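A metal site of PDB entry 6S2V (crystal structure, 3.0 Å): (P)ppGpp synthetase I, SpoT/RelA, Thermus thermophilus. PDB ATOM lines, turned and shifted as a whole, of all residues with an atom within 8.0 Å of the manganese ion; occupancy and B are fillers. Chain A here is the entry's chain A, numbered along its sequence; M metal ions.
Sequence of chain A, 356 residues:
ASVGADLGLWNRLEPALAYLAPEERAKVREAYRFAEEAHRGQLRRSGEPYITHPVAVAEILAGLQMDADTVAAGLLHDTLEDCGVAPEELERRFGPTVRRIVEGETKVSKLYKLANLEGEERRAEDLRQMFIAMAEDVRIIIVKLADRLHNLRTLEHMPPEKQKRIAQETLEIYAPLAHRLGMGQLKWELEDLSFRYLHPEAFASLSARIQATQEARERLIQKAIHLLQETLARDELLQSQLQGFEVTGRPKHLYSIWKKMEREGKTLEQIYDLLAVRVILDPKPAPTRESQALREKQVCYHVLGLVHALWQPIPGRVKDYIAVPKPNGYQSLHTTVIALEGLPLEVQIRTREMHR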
ATOM      1  N   HIS A  39     -11.784  -6.025  18.207  1.00  0.00           N
ATOM      2  CA  HIS A  39     -10.557  -5.293  18.556  1.00  0.00           C
ATOM      3  C   HIS A  39      -9.323  -6.182  18.690  1.00  0.00           C
ATOM      4  O   HIS A  39      -8.308  -5.722  19.236  1.00  0.00           O
ATOM      5  CB  HIS A  39     -10.770  -4.431  19.820  1.00  0.00           C
ATOM      6  CG  HIS A  39     -11.800  -3.358  19.651  1.00  0.00           C
ATOM      7  ND1 HIS A  39     -11.605  -2.317  18.770  1.00  0.00           N
ATOM      8  CD2 HIS A  39     -13.006  -3.209  20.262  1.00  0.00           C
ATOM      9  CE1 HIS A  39     -12.699  -1.557  18.877  1.00  0.00           C
ATOM     10  NE2 HIS A  39     -13.561  -2.052  19.753  1.00  0.00           N
ATOM     11  N   ARG A  45      -2.296   4.063  21.672  1.00  0.00           N
ATOM     12  CA  ARG A  45      -1.094   4.918  21.577  1.00  0.00           C
ATOM     13  C   ARG A  45      -0.032   4.280  22.502  1.00  0.00           C
ATOM     14  O   ARG A  45       1.109   4.063  22.090  1.00  0.00           O
ATOM     15  CB  ARG A  45      -1.406   6.374  21.975  1.00  0.00           C
ATOM     16  CG  ARG A  45      -2.246   7.176  20.971  1.00  0.00           C
ATOM     17  CD  ARG A  45      -3.741   7.120  21.278  1.00  0.00           C
ATOM     18  NE  ARG A  45      -4.421   6.069  20.519  1.00  0.00           N
ATOM     19  CZ  ARG A  45      -5.383   5.272  21.002  1.00  0.00           C
ATOM     20  NH1 ARG A  45      -5.936   4.352  20.237  1.00  0.00           N
ATOM     21  NH2 ARG A  45      -5.774   5.394  22.266  1.00  0.00           N
ATOM     22  N   TYR A  50      -6.136  -2.647  22.335  1.00  0.00           N
ATOM     23  CA  TYR A  50      -7.297  -1.752  22.289  1.00  0.00           C
ATOM     24  C   TYR A  50      -8.422  -2.136  23.224  1.00  0.00           C
ATOM     25  O   TYR A  50      -8.975  -1.237  23.842  1.00  0.00           O
ATOM     26  CB  TYR A  50      -7.837  -1.551  20.864  1.00  0.00           C
ATOM     27  CG  TYR A  50      -8.610  -0.250  20.709  1.00  0.00           C
ATOM     28  CD1 TYR A  50      -7.955   0.943  20.408  1.00  0.00           C
ATOM     29  CD2 TYR A  50      -9.993  -0.210  20.864  1.00  0.00           C
ATOM     30  CE1 TYR A  50      -8.663   2.143  20.260  1.00  0.00           C
ATOM     31  CE2 TYR A  50     -10.713   0.981  20.730  1.00  0.00           C
ATOM     32  CZ  TYR A  50     -10.036   2.153  20.420  1.00  0.00           C
ATOM     33  OH  TYR A  50     -10.733   3.323  20.277  1.00  0.00           O
ATOM     34  N   HIS A  53      -9.360  -0.099  26.389  1.00  0.00           N
ATOM     35  CA  HIS A  53     -10.143   1.131  26.299  1.00  0.00           C
ATOM     36  C   HIS A  53     -11.655   0.870  26.481  1.00  0.00           C
ATOM     37  O   HIS A  53     -12.170   1.347  27.489  1.00  0.00           O
ATOM     38  CB  HIS A  53      -9.831   1.952  25.025  1.00  0.00           C
ATOM     39  CG  HIS A  53     -10.787   3.069  24.756  1.00  0.00           C
ATOM     40  ND1 HIS A  53     -10.912   4.137  25.614  1.00  0.00           N
ATOM     41  CD2 HIS A  53     -11.626   3.264  23.705  1.00  0.00           C
ATOM     42  CE1 HIS A  53     -11.823   4.919  25.083  1.00  0.00           C
ATOM     43  NE2 HIS A  53     -12.274   4.440  23.933  1.00  0.00           N
ATOM     44  N   PRO A  54     -12.379   0.084  25.616  1.00  0.00           N
ATOM     45  CA  PRO A  54     -13.810  -0.142  25.867  1.00  0.00           C
ATOM     46  C   PRO A  54     -14.140  -0.754  27.238  1.00  0.00           C
ATOM     47  O   PRO A  54     -15.188  -0.426  27.798  1.00  0.00           O
ATOM     48  CB  PRO A  54     -14.230  -1.017  24.691  1.00  0.00           C
ATOM     49  CG  PRO A  54     -13.254  -0.696  23.604  1.00  0.00           C
ATOM     50  CD  PRO A  54     -11.974  -0.581  24.361  1.00  0.00           C
ATOM     51  N   VAL A  57     -14.002   2.076  29.688  1.00  0.00           N
ATOM     52  CA  VAL A  57     -15.207   2.885  29.435  1.00  0.00           C
ATOM     53  C   VAL A  57     -16.406   2.195  30.106  1.00  0.00           C
ATOM     54  O   VAL A  57     -17.182   2.885  30.770  1.00  0.00           O
ATOM     55  CB  VAL A  57     -15.412   3.180  27.928  1.00  0.00           C
ATOM     56  CG1 VAL A  57     -16.711   3.950  27.682  1.00  0.00           C
ATOM     57  CG2 VAL A  57     -14.229   3.948  27.356  1.00  0.00           C
ATOM     58  N   GLY A  74     -20.929   0.488  25.818  1.00  0.00           N
ATOM     59  CA  GLY A  74     -19.618   1.009  26.208  1.00  0.00           C
ATOM     60  C   GLY A  74     -18.511   0.064  25.786  1.00  0.00           C
ATOM     61  O   GLY A  74     -17.432   0.499  25.394  1.00  0.00           O
ATOM     62  N   HIS A  77     -18.737   0.646  21.684  1.00  0.00           N
ATOM     63  CA  HIS A  77     -18.757   2.015  21.116  1.00  0.00           C
ATOM     64  C   HIS A  77     -17.725   2.280  19.998  1.00  0.00           C
ATOM     65  O   HIS A  77     -17.912   3.207  19.201  1.00  0.00           O
ATOM     66  CB  HIS A  77     -18.641   3.079  22.230  1.00  0.00           C
ATOM     67  CG  HIS A  77     -17.260   3.265  22.762  1.00  0.00           C
ATOM     68  ND1 HIS A  77     -16.721   2.413  23.710  1.00  0.00           N
ATOM     69  CD2 HIS A  77     -16.326   4.198  22.453  1.00  0.00           C
ATOM     70  CE1 HIS A  77     -15.503   2.859  23.962  1.00  0.00           C
ATOM     71  NE2 HIS A  77     -15.212   3.917  23.213  1.00  0.00           N
ATOM     72  N   ASP A  78     -16.644   1.471  19.935  1.00  0.00           N
ATOM     73  CA  ASP A  78     -15.612   1.644  18.922  1.00  0.00           C
ATOM     74  C   ASP A  78     -15.551   0.472  17.932  1.00  0.00           C
ATOM     75  O   ASP A  78     -14.691   0.462  17.061  1.00  0.00           O
ATOM     76  CB  ASP A  78     -14.253   1.950  19.578  1.00  0.00           C
ATOM     77  CG  ASP A  78     -14.099   3.398  20.024  1.00  0.00           C
ATOM     78  OD1 ASP A  78     -14.672   4.303  19.357  1.00  0.00           O
ATOM     79  OD2 ASP A  78     -13.411   3.622  21.037  1.00  0.00           O
ATOM     80  N   THR A  79     -16.508  -0.460  18.006  1.00  0.00           N
ATOM     81  CA  THR A  79     -16.590  -1.574  17.059  1.00  0.00           C
ATOM     82  C   THR A  79     -17.080  -1.091  15.675  1.00  0.00           C
ATOM     83  O   THR A  79     -16.956  -1.816  14.712  1.00  0.00           O
ATOM     84  CB  THR A  79     -17.407  -2.783  17.610  1.00  0.00           C
ATOM     85  OG1 THR A  79     -18.761  -2.381  17.827  1.00  0.00           O
ATOM     86  CG2 THR A  79     -16.782  -3.442  18.847  1.00  0.00           C
ATOM     87  N   GLU A  81     -16.538   2.571  14.646  1.00  0.00           N
ATOM     88  CA  GLU A  81     -15.560   3.606  14.340  1.00  0.00           C
ATOM     89  C   GLU A  81     -14.122   3.036  14.210  1.00  0.00           C
ATOM     90  O   GLU A  81     -13.614   2.885  13.096  1.00  0.00           O
ATOM     91  CB  GLU A  81     -15.646   4.759  15.371  1.00  0.00           C
ATOM     92  N   ASP A  82     -13.517   2.671  15.338  1.00  0.00           N
ATOM     93  CA  ASP A  82     -12.127   2.146  15.331  1.00  0.00           C
ATOM     94  C   ASP A  82     -11.993   0.946  14.390  1.00  0.00           C
ATOM     95  O   ASP A  82     -11.213   1.059  13.421  1.00  0.00           O
ATOM     96  CB  ASP A  82     -11.649   1.820  16.751  1.00  0.00           C
ATOM     97  N   VAL A 143     -22.138   7.740  27.260  1.00  0.00           N
ATOM     98  CA  VAL A 143     -21.065   6.888  26.718  1.00  0.00           C
ATOM     99  C   VAL A 143     -19.958   7.764  26.118  1.00  0.00           C
ATOM    100  O   VAL A 143     -18.779   7.523  26.414  1.00  0.00           O
ATOM    101  CB  VAL A 143     -21.496   5.713  25.784  1.00  0.00           C
ATOM    102  CG1 VAL A 143     -22.509   4.775  26.446  1.00  0.00           C
ATOM    103  CG2 VAL A 143     -21.953   6.158  24.391  1.00  0.00           C
ATOM    104  N   LYS A 144     -20.338   8.815  25.348  1.00  0.00           N
ATOM    105  CA  LYS A 144     -19.396   9.775  24.744  1.00  0.00           C
ATOM    106  C   LYS A 144     -18.512  10.360  25.865  1.00  0.00           C
ATOM    107  O   LYS A 144     -17.280  10.435  25.723  1.00  0.00           O
ATOM    108  CB  LYS A 144     -20.160  10.930  24.022  1.00  0.00           C
ATOM    109  CG  LYS A 144     -21.052  10.535  22.839  1.00  0.00           C
ATOM    110  N   ALA A 146     -17.999   9.129  29.073  1.00  0.00           N
ATOM    111  CA  ALA A 146     -17.199   8.087  29.720  1.00  0.00           C
ATOM    112  C   ALA A 146     -15.956   7.858  28.890  1.00  0.00           C
ATOM    113  O   ALA A 146     -14.862   7.818  29.444  1.00  0.00           O
ATOM    114  CB  ALA A 146     -18.009   6.791  29.851  1.00  0.00           C
ATOM    115  N   ASP A 147     -16.133   7.776  27.550  1.00  0.00           N
ATOM    116  CA  ASP A 147     -15.070   7.585  26.562  1.00  0.00           C
ATOM    117  C   ASP A 147     -14.045   8.731  26.637  1.00  0.00           C
ATOM    118  O   ASP A 147     -12.850   8.465  26.747  1.00  0.00           O
ATOM    119  CB  ASP A 147     -15.691   7.480  25.157  1.00  0.00           C
ATOM    120  CG  ASP A 147     -14.751   7.699  23.982  1.00  0.00           C
ATOM    121  OD1 ASP A 147     -14.914   8.709  23.265  1.00  0.00           O
ATOM    122  OD2 ASP A 147     -13.865   6.857  23.776  1.00  0.00           O
ATOM    123  N   ARG A 148     -14.545   9.987  26.599  1.00  0.00           N
ATOM    124  CA  ARG A 148     -13.697  11.176  26.630  1.00  0.00           C
ATOM    125  C   ARG A 148     -12.929  11.276  27.939  1.00  0.00           C
ATOM    126  O   ARG A 148     -11.743  11.588  27.916  1.00  0.00           O
ATOM    127  CB  ARG A 148     -14.496  12.446  26.323  1.00  0.00           C
ATOM    128  CG  ARG A 148     -13.647  13.729  26.220  1.00  0.00           C
ATOM    129  CD  ARG A 148     -12.365  13.597  25.400  1.00  0.00           C
ATOM    130  NE  ARG A 148     -12.598  13.510  23.958  1.00  0.00           N
ATOM    131  CZ  ARG A 148     -12.445  14.531  23.130  1.00  0.00           C
ATOM    132  NH1 ARG A 148     -12.128  15.725  23.586  1.00  0.00           N
ATOM    133  NH2 ARG A 148     -12.667  14.369  21.831  1.00  0.00           N
ATOM    134  N   HIS A 150     -11.998   8.803  29.891  1.00  0.00           N
ATOM    135  CA  HIS A 150     -10.931   7.814  29.876  1.00  0.00           C
ATOM    136  C   HIS A 150      -9.777   8.239  28.981  1.00  0.00           C
ATOM    137  O   HIS A 150      -8.631   8.110  29.400  1.00  0.00           O
ATOM    138  CB  HIS A 150     -11.438   6.418  29.503  1.00  0.00           C
ATOM    139  CG  HIS A 150     -10.327   5.410  29.317  1.00  0.00           C
ATOM    140  ND1 HIS A 150     -10.309   4.577  28.228  1.00  0.00           N
ATOM    141  CD2 HIS A 150      -9.235   5.163  30.079  1.00  0.00           C
ATOM    142  CE1 HIS A 150      -9.207   3.853  28.351  1.00  0.00           C
ATOM    143  NE2 HIS A 150      -8.529   4.160  29.456  1.00  0.00           N
ATOM    144  N   ASN A 151     -10.056   8.752  27.769  1.00  0.00           N
ATOM    145  CA  ASN A 151      -9.015   9.211  26.852  1.00  0.00           C
ATOM    146  C   ASN A 151      -8.115  10.244  27.545  1.00  0.00           C
ATOM    147  O   ASN A 151      -6.888  10.117  27.506  1.00  0.00           O
ATOM    148  CB  ASN A 151      -9.631   9.796  25.573  1.00  0.00           C
ATOM    149  CG  ASN A 151      -9.714   8.828  24.419  1.00  0.00           C
ATOM    150  OD1 ASN A 151      -9.955   7.628  24.582  1.00  0.00           O
ATOM    151  ND2 ASN A 151      -9.491   9.323  23.205  1.00  0.00           N
HETATM  152 MN    MN M   1     -13.453   5.335  22.523  1.00  0.00          MN
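A ring nitrogen (ND1) of His 53 is in hydrogen-bond range of a ring nitrogen (ND1) of His 150 (2.7 Å).
A ring nitrogen (ND1) of His 77 lies within hydrogen-bond range of the backbone carbonyl oxygen (O) of Gly 74, at 2.6 Å.
The side-chain carboxylate of Asp 78 sits close to the side-chain hydroxyl of Tyr 50, at 2.8 Å.
Within 4 Å of the manganese ion: His 53, His 77, Asp 78 and Asp 147.
The manganese ion is bound by OD2 of Asp 147 (2.0 Å), NE2 of His 53 (2.0 Å), OD2 of Asp 78 (2.3 Å) and NE2 of His 77 (2.4 Å).
The manganese ion has four donor atoms within binding distance.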
